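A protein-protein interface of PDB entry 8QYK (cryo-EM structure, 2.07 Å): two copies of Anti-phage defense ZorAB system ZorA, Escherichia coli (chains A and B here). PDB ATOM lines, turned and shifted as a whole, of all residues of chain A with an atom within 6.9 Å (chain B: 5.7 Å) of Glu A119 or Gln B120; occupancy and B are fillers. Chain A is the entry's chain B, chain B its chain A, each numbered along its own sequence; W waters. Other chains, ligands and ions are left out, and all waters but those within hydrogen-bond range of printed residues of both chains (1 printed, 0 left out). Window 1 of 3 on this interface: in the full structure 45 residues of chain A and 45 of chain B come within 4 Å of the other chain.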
ATOM      1  N   ALA A 114       9.428  -0.515  27.164  1.00  0.00           N
ATOM      2  CA  ALA A 114       9.215   0.820  27.706  1.00  0.00           C
ATOM      3  C   ALA A 114       9.992   1.067  28.991  1.00  0.00           C
ATOM      4  O   ALA A 114      10.247   2.228  29.323  1.00  0.00           O
ATOM      5  CB  ALA A 114       7.726   1.059  27.957  1.00  0.00           C
ATOM      6  N   PHE A 116      13.070   0.499  29.435  1.00  0.00           N
ATOM      7  CA  PHE A 116      14.390   0.980  29.041  1.00  0.00           C
ATOM      8  C   PHE A 116      14.334   2.107  28.027  1.00  0.00           C
ATOM      9  O   PHE A 116      15.129   3.044  28.111  1.00  0.00           O
ATOM     10  CB  PHE A 116      15.227  -0.178  28.483  1.00  0.00           C
ATOM     11  CG  PHE A 116      15.244  -1.381  29.370  1.00  0.00           C
ATOM     12  CD1 PHE A 116      16.143  -1.470  30.416  1.00  0.00           C
ATOM     13  CD2 PHE A 116      14.343  -2.413  29.177  1.00  0.00           C
ATOM     14  CE1 PHE A 116      16.153  -2.570  31.242  1.00  0.00           C
ATOM     15  CE2 PHE A 116      14.350  -3.514  30.003  1.00  0.00           C
ATOM     16  CZ  PHE A 116      15.253  -3.591  31.036  1.00  0.00           C
ATOM     17  N   PHE A 117      13.417   2.039  27.065  1.00  0.00           N
ATOM     18  CA  PHE A 117      13.164   3.150  26.149  1.00  0.00           C
ATOM     19  C   PHE A 117      12.006   3.997  26.679  1.00  0.00           C
ATOM     20  O   PHE A 117      10.940   4.109  26.079  1.00  0.00           O
ATOM     21  CB  PHE A 117      12.883   2.630  24.745  1.00  0.00           C
ATOM     22  CG  PHE A 117      14.027   1.871  24.137  1.00  0.00           C
ATOM     23  CD1 PHE A 117      14.202   0.524  24.403  1.00  0.00           C
ATOM     24  CD2 PHE A 117      14.917   2.501  23.289  1.00  0.00           C
ATOM     25  CE1 PHE A 117      15.245  -0.174  23.843  1.00  0.00           C
ATOM     26  CE2 PHE A 117      15.963   1.806  22.721  1.00  0.00           C
ATOM     27  CZ  PHE A 117      16.125   0.467  22.998  1.00  0.00           C
ATOM     28  N   SER A 118      12.249   4.594  27.839  1.00  0.00           N
ATOM     29  CA  SER A 118      11.217   5.272  28.603  1.00  0.00           C
ATOM     30  C   SER A 118      10.941   6.663  28.042  1.00  0.00           C
ATOM     31  O   SER A 118      11.724   7.225  27.273  1.00  0.00           O
ATOM     32  CB  SER A 118      11.625   5.374  30.069  1.00  0.00           C
ATOM     33  OG  SER A 118      12.778   6.183  30.211  1.00  0.00           O
ATOM     34  N   GLU A 119       9.803   7.221  28.455  1.00  0.00           N
ATOM     35  CA  GLU A 119       9.455   8.577  28.053  1.00  0.00           C
ATOM     36  C   GLU A 119      10.421   9.599  28.638  1.00  0.00           C
ATOM     37  O   GLU A 119      10.799  10.555  27.957  1.00  0.00           O
ATOM     38  CB  GLU A 119       8.014   8.892  28.454  1.00  0.00           C
ATOM     39  CG  GLU A 119       6.988   8.104  27.661  1.00  0.00           C
ATOM     40  CD  GLU A 119       5.563   8.389  28.087  1.00  0.00           C
ATOM     41  OE1 GLU A 119       5.367   9.163  29.045  1.00  0.00           O
ATOM     42  OE2 GLU A 119       4.635   7.835  27.462  1.00  0.00           O
ATOM     43  N   GLN A 120      10.841   9.416  29.892  1.00  0.00           N
ATOM     44  CA  GLN A 120      11.761  10.374  30.499  1.00  0.00           C
ATOM     45  C   GLN A 120      13.095  10.409  29.765  1.00  0.00           C
ATOM     46  O   GLN A 120      13.608  11.487  29.449  1.00  0.00           O
ATOM     47  CB  GLN A 120      11.972  10.047  31.978  1.00  0.00           C
ATOM     48  CG  GLN A 120      13.259  10.627  32.551  1.00  0.00           C
ATOM     49  CD  GLN A 120      13.210  10.836  34.051  1.00  0.00           C
ATOM     50  OE1 GLN A 120      12.850   9.935  34.806  1.00  0.00           O
ATOM     51  NE2 GLN A 120      13.581  12.033  34.493  1.00  0.00           N
ATOM     52  N   GLN A 121      13.664   9.242  29.468  1.00  0.00           N
ATOM     53  CA  GLN A 121      14.987   9.208  28.855  1.00  0.00           C
ATOM     54  C   GLN A 121      14.959   9.592  27.382  1.00  0.00           C
ATOM     55  O   GLN A 121      15.927  10.171  26.885  1.00  0.00           O
ATOM     56  CB  GLN A 121      15.608   7.823  29.031  1.00  0.00           C
ATOM     57  CG  GLN A 121      15.927   7.481  30.477  1.00  0.00           C
ATOM     58  CD  GLN A 121      16.520   6.101  30.629  1.00  0.00           C
ATOM     59  OE1 GLN A 121      16.638   5.357  29.659  1.00  0.00           O
ATOM     60  NE2 GLN A 121      16.897   5.748  31.851  1.00  0.00           N
ATOM     61  N   LEU A 122      13.869   9.300  26.672  1.00  0.00           N
ATOM     62  CA  LEU A 122      13.831   9.500  25.232  1.00  0.00           C
ATOM     63  C   LEU A 122      13.118  10.773  24.799  1.00  0.00           C
ATOM     64  O   LEU A 122      13.321  11.212  23.664  1.00  0.00           O
ATOM     65  CB  LEU A 122      13.167   8.297  24.544  1.00  0.00           C
ATOM     66  CG  LEU A 122      14.106   7.184  24.067  1.00  0.00           C
ATOM     67  CD1 LEU A 122      14.831   6.527  25.231  1.00  0.00           C
ATOM     68  CD2 LEU A 122      13.355   6.148  23.255  1.00  0.00           C
ATOM     69  N   VAL A 123      12.298  11.374  25.660  1.00  0.00           N
ATOM     70  CA  VAL A 123      11.541  12.568  25.306  1.00  0.00           C
ATOM     71  C   VAL A 123      11.783  13.662  26.338  1.00  0.00           C
ATOM     72  O   VAL A 123      12.234  14.759  25.998  1.00  0.00           O
ATOM     73  CB  VAL A 123      10.036  12.261  25.188  1.00  0.00           C
ATOM     74  CG1 VAL A 123       9.284  13.473  24.666  1.00  0.00           C
ATOM     75  CG2 VAL A 123       9.794  11.053  24.294  1.00  0.00           C
ATOM     76  N   ASP A 124      11.496  13.360  27.608  1.00  0.00           N
ATOM     77  CA  ASP A 124      11.435  14.400  28.632  1.00  0.00           C
ATOM     78  C   ASP A 124      12.784  15.079  28.841  1.00  0.00           C
ATOM     79  O   ASP A 124      12.874  16.311  28.807  1.00  0.00           O
ATOM     80  CB  ASP A 124      10.928  13.809  29.947  1.00  0.00           C
ATOM     81  CG  ASP A 124       9.485  13.352  29.861  1.00  0.00           C
ATOM     82  OD1 ASP A 124       8.720  13.937  29.067  1.00  0.00           O
ATOM     83  OD2 ASP A 124       9.112  12.409  30.589  1.00  0.00           O
ATOM     84  N   ILE A 125      13.836  14.302  29.066  1.00  0.00           N
ATOM     85  CA  ILE A 125      15.172  14.852  29.281  1.00  0.00           C
ATOM     86  C   ILE A 125      15.722  15.471  27.996  1.00  0.00           C
ATOM     87  O   ILE A 125      16.232  16.599  28.046  1.00  0.00           O
ATOM     88  CB  ILE A 125      16.117  13.785  29.855  1.00  0.00           C
ATOM     89  CG1 ILE A 125      15.825  13.585  31.343  1.00  0.00           C
ATOM     90  CG2 ILE A 125      17.568  14.178  29.645  1.00  0.00           C
ATOM     91  CD1 ILE A 125      16.482  12.369  31.938  1.00  0.00           C
ATOM     92  N   PRO A 126      15.660  14.798  26.835  1.00  0.00           N
ATOM     93  CA  PRO A 126      16.158  15.448  25.608  1.00  0.00           C
ATOM     94  C   PRO A 126      15.450  16.749  25.280  1.00  0.00           C
ATOM     95  O   PRO A 126      16.086  17.686  24.783  1.00  0.00           O
ATOM     96  CB  PRO A 126      15.911  14.388  24.527  1.00  0.00           C
ATOM     97  CG  PRO A 126      15.890  13.118  25.254  1.00  0.00           C
ATOM     98  CD  PRO A 126      15.249  13.408  26.564  1.00  0.00           C
ATOM     99  N   SER A 205       4.988  12.901  20.488  1.00  0.00           N
ATOM    100  CA  SER A 205       6.178  12.170  20.902  1.00  0.00           C
ATOM    101  C   SER A 205       5.808  10.929  21.695  1.00  0.00           C
ATOM    102  O   SER A 205       6.346   9.845  21.451  1.00  0.00           O
ATOM    103  CB  SER A 205       7.088  13.073  21.734  1.00  0.00           C
ATOM    104  OG  SER A 205       7.486  14.220  21.013  1.00  0.00           O
ATOM    105  N   TYR A 206       4.883  11.066  22.648  1.00  0.00           N
ATOM    106  CA  TYR A 206       4.470   9.915  23.439  1.00  0.00           C
ATOM    107  C   TYR A 206       3.797   8.864  22.568  1.00  0.00           C
ATOM    108  O   TYR A 206       4.047   7.665  22.732  1.00  0.00           O
ATOM    109  CB  TYR A 206       3.542  10.356  24.570  1.00  0.00           C
ATOM    110  CG  TYR A 206       4.248  11.068  25.699  1.00  0.00           C
ATOM    111  CD1 TYR A 206       5.629  11.194  25.708  1.00  0.00           C
ATOM    112  CD2 TYR A 206       3.535  11.616  26.755  1.00  0.00           C
ATOM    113  CE1 TYR A 206       6.278  11.846  26.731  1.00  0.00           C
ATOM    114  CE2 TYR A 206       4.179  12.268  27.786  1.00  0.00           C
ATOM    115  CZ  TYR A 206       5.551  12.378  27.768  1.00  0.00           C
ATOM    116  OH  TYR A 206       6.207  13.026  28.788  1.00  0.00           O
ATOM    117  N   LYS A 207       2.951   9.296  21.629  1.00  0.00           N
ATOM    118  CA  LYS A 207       2.285   8.344  20.744  1.00  0.00           C
ATOM    119  C   LYS A 207       3.291   7.557  19.910  1.00  0.00           C
ATOM    120  O   LYS A 207       3.205   6.324  19.804  1.00  0.00           O
ATOM    121  CB  LYS A 207       1.306   9.086  19.840  1.00  0.00           C
ATOM    122  CG  LYS A 207       0.716   8.241  18.735  1.00  0.00           C
ATOM    123  CD  LYS A 207      -0.114   9.090  17.796  1.00  0.00           C
ATOM    124  CE  LYS A 207      -0.665   8.268  16.646  1.00  0.00           C
ATOM    125  NZ  LYS A 207      -1.464   9.099  15.711  1.00  0.00           N
ATOM    126  N   LEU A 209       6.549   7.152  20.444  1.00  0.00           N
ATOM    127  CA  LEU A 209       7.366   6.312  21.314  1.00  0.00           C
ATOM    128  C   LEU A 209       6.610   5.057  21.732  1.00  0.00           C
ATOM    129  O   LEU A 209       7.207   3.983  21.855  1.00  0.00           O
ATOM    130  CB  LEU A 209       7.819   7.105  22.540  1.00  0.00           C
ATOM    131  CG  LEU A 209       8.653   6.344  23.573  1.00  0.00           C
ATOM    132  CD1 LEU A 209       9.818   5.613  22.925  1.00  0.00           C
ATOM    133  CD2 LEU A 209       9.146   7.285  24.656  1.00  0.00           C
ATOM    134  N   GLU A 210       5.298   5.168  21.954  1.00  0.00           N
ATOM    135  CA  GLU A 210       4.500   3.978  22.226  1.00  0.00           C
ATOM    136  C   GLU A 210       4.507   3.029  21.038  1.00  0.00           C
ATOM    137  O   GLU A 210       4.627   1.813  21.208  1.00  0.00           O
ATOM    138  CB  GLU A 210       3.069   4.368  22.591  1.00  0.00           C
ATOM    139  CG  GLU A 210       2.299   3.277  23.318  1.00  0.00           C
ATOM    140  CD  GLU A 210       1.800   2.184  22.388  1.00  0.00           C
ATOM    141  OE1 GLU A 210       1.350   2.509  21.270  1.00  0.00           O
ATOM    142  OE2 GLU A 210       1.873   0.999  22.768  1.00  0.00           O
ATOM    143  N   SER B 118      -3.733  -1.042  28.984  1.00  0.00           N
ATOM    144  CA  SER B 118      -3.506   0.047  29.920  1.00  0.00           C
ATOM    145  C   SER B 118      -4.353   1.265  29.570  1.00  0.00           C
ATOM    146  O   SER B 118      -4.841   1.422  28.449  1.00  0.00           O
ATOM    147  CB  SER B 118      -2.030   0.443  29.942  1.00  0.00           C
ATOM    148  OG  SER B 118      -1.630   1.011  28.709  1.00  0.00           O
ATOM    149  N   GLU B 119      -4.521   2.137  30.563  1.00  0.00           N
ATOM    150  CA  GLU B 119      -5.213   3.397  30.328  1.00  0.00           C
ATOM    151  C   GLU B 119      -4.453   4.259  29.331  1.00  0.00           C
ATOM    152  O   GLU B 119      -5.064   4.916  28.482  1.00  0.00           O
ATOM    153  CB  GLU B 119      -5.425   4.143  31.644  1.00  0.00           C
ATOM    154  CG  GLU B 119      -6.446   3.488  32.555  1.00  0.00           C
ATOM    155  CD  GLU B 119      -6.626   4.221  33.868  1.00  0.00           C
ATOM    156  OE1 GLU B 119      -5.757   5.047  34.216  1.00  0.00           O
ATOM    157  OE2 GLU B 119      -7.640   3.971  34.551  1.00  0.00           O
ATOM    158  N   GLN B 120      -3.121   4.259  29.404  1.00  0.00           N
ATOM    159  CA  GLN B 120      -2.334   5.014  28.436  1.00  0.00           C
ATOM    160  C   GLN B 120      -2.646   4.563  27.015  1.00  0.00           C
ATOM    161  O   GLN B 120      -3.264   5.306  26.246  1.00  0.00           O
ATOM    162  CB  GLN B 120      -0.841   4.874  28.732  1.00  0.00           C
ATOM    163  CG  GLN B 120      -0.008   5.993  28.129  1.00  0.00           C
ATOM    164  CD  GLN B 120       1.419   5.584  27.821  1.00  0.00           C
ATOM    165  OE1 GLN B 120       1.752   4.399  27.796  1.00  0.00           O
ATOM    166  NE2 GLN B 120       2.269   6.569  27.571  1.00  0.00           N
ATOM    167  N   GLN B 121      -2.334   3.303  26.703  1.00  0.00           N
ATOM    168  CA  GLN B 121      -2.363   2.818  25.326  1.00  0.00           C
ATOM    169  C   GLN B 121      -3.772   2.807  24.747  1.00  0.00           C
ATOM    170  O   GLN B 121      -3.951   2.972  23.536  1.00  0.00           O
ATOM    171  CB  GLN B 121      -1.758   1.416  25.269  1.00  0.00           C
ATOM    172  CG  GLN B 121      -0.251   1.406  25.143  1.00  0.00           C
ATOM    173  CD  GLN B 121       0.375   0.177  25.764  1.00  0.00           C
ATOM    174  OE1 GLN B 121       0.055  -0.192  26.892  1.00  0.00           O
ATOM    175  NE2 GLN B 121       1.273  -0.465  25.029  1.00  0.00           N
ATOM    176  N   LEU B 122      -4.781   2.585  25.580  1.00  0.00           N
ATOM    177  CA  LEU B 122      -6.140   2.443  25.079  1.00  0.00           C
ATOM    178  C   LEU B 122      -6.975   3.707  25.215  1.00  0.00           C
ATOM    179  O   LEU B 122      -8.032   3.797  24.585  1.00  0.00           O
ATOM    180  CB  LEU B 122      -6.850   1.283  25.787  1.00  0.00           C
ATOM    181  CG  LEU B 122      -6.611  -0.121  25.222  1.00  0.00           C
ATOM    182  CD1 LEU B 122      -5.180  -0.574  25.434  1.00  0.00           C
ATOM    183  CD2 LEU B 122      -7.574  -1.118  25.843  1.00  0.00           C
ATOM    184  N   VAL B 123      -6.546   4.681  26.012  1.00  0.00           N
ATOM    185  CA  VAL B 123      -7.346   5.884  26.212  1.00  0.00           C
ATOM    186  C   VAL B 123      -6.516   7.135  25.957  1.00  0.00           C
ATOM    187  O   VAL B 123      -6.868   7.962  25.110  1.00  0.00           O
ATOM    188  CB  VAL B 123      -7.953   5.913  27.627  1.00  0.00           C
ATOM    189  CG1 VAL B 123      -8.706   7.205  27.849  1.00  0.00           C
ATOM    190  CG2 VAL B 123      -8.864   4.720  27.847  1.00  0.00           C
ATOM    191  N   ASP B 124      -5.395   7.266  26.667  1.00  0.00           N
ATOM    192  CA  ASP B 124      -4.731   8.562  26.770  1.00  0.00           C
ATOM    193  C   ASP B 124      -4.061   8.951  25.462  1.00  0.00           C
ATOM    194  O   ASP B 124      -4.069  10.126  25.078  1.00  0.00           O
ATOM    195  CB  ASP B 124      -3.709   8.530  27.902  1.00  0.00           C
ATOM    196  CG  ASP B 124      -4.354   8.368  29.260  1.00  0.00           C
ATOM    197  OD1 ASP B 124      -5.581   8.565  29.372  1.00  0.00           O
ATOM    198  OD2 ASP B 124      -3.631   8.036  30.215  1.00  0.00           O
ATOM    199  N   ILE B 125      -3.465   7.987  24.775  1.00  0.00           N
ATOM    200  CA  ILE B 125      -2.790   8.242  23.509  1.00  0.00           C
ATOM    201  C   ILE B 125      -3.809   8.370  22.379  1.00  0.00           C
ATOM    202  O   ILE B 125      -3.714   9.325  21.595  1.00  0.00           O
ATOM    203  CB  ILE B 125      -1.740   7.158  23.218  1.00  0.00           C
ATOM    204  CG1 ILE B 125      -0.491   7.416  24.060  1.00  0.00           C
ATOM    205  CG2 ILE B 125      -1.409   7.114  21.738  1.00  0.00           C
ATOM    206  CD1 ILE B 125       0.453   6.257  24.112  1.00  0.00           C
ATOM    207  N   PRO B 126      -4.789   7.466  22.233  1.00  0.00           N
ATOM    208  CA  PRO B 126      -5.799   7.688  21.186  1.00  0.00           C
ATOM    209  C   PRO B 126      -6.572   8.982  21.361  1.00  0.00           C
ATOM    210  O   PRO B 126      -6.926   9.619  20.363  1.00  0.00           O
ATOM    211  CB  PRO B 126      -6.709   6.455  21.297  1.00  0.00           C
ATOM    212  CG  PRO B 126      -6.393   5.838  22.590  1.00  0.00           C
ATOM    213  CD  PRO B 126      -4.970   6.149  22.870  1.00  0.00           C
HETATM  214  O   HOH W   1       4.456  -0.270  24.330  1.00  0.00           O
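NE2 of Gln B121 lies within hydrogen-bond range of OE2 of Glu A210, 2.8 Å away. NE2 of Gln B120 sits at hydrogen-bond distance from OE2 of Glu A119 (2.7 Å).
The backbone NH of Asp A124 sits at hydrogen-bond distance from the backbone carbonyl oxygen of Glu A119 (2.9 Å). OG of Ser B118 is in hydrogen-bond range of OE1 of Gln B121 (2.8 Å). The backbone carbonyl oxygen (O) of Gln B120 sits at hydrogen-bond distance from the backbone NH (N) of Ile B125, at 3.1 Å.
Ile B125 touches Lys A207 (CG2 to CG, 3.8 Å). Glu A210 touches Ile B125.
Of the printed residues of chain A, Gln B120 touches Glu A119. Of the printed residues of chain B, Lys A207 touches Ile B125. Of the printed residues of chain B, Glu A210 touches Gln B121 and Ile B125. Of the printed residues of chain A, Ile B125 touches Lys A207 and Glu A210. Printed residues of chain A within 4 Å of Gln B121: Glu A210. Tyr A206 touches none of the printed residues of chain B. Ser A118 touches none of the printed residues of chain B.
Printed residues of chain A that touch a printed residue of chain B: Glu A119, Lys A207 and Glu A210. Hydrophobic or aromatic side chains of chain B that line the printed part of chain A: Ile B125. Among the printed residues, 4 pairs touch across the chains. Among the printed residues, no Asp or Glu carboxylate lies within 4 Å of a Lys or Arg side-chain nitrogen of the other chain.
Glu A119 touches Gln B120, but with the chains exchanged Gln A120 does not touch Glu B119 (16.1 Å). Positions printed for both chains: 118, 119, 120, 121, 122, 123, 124, 125 and 126.
Water W1 bridges NE2 of Gln B121 and OE2 of Glu A210.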
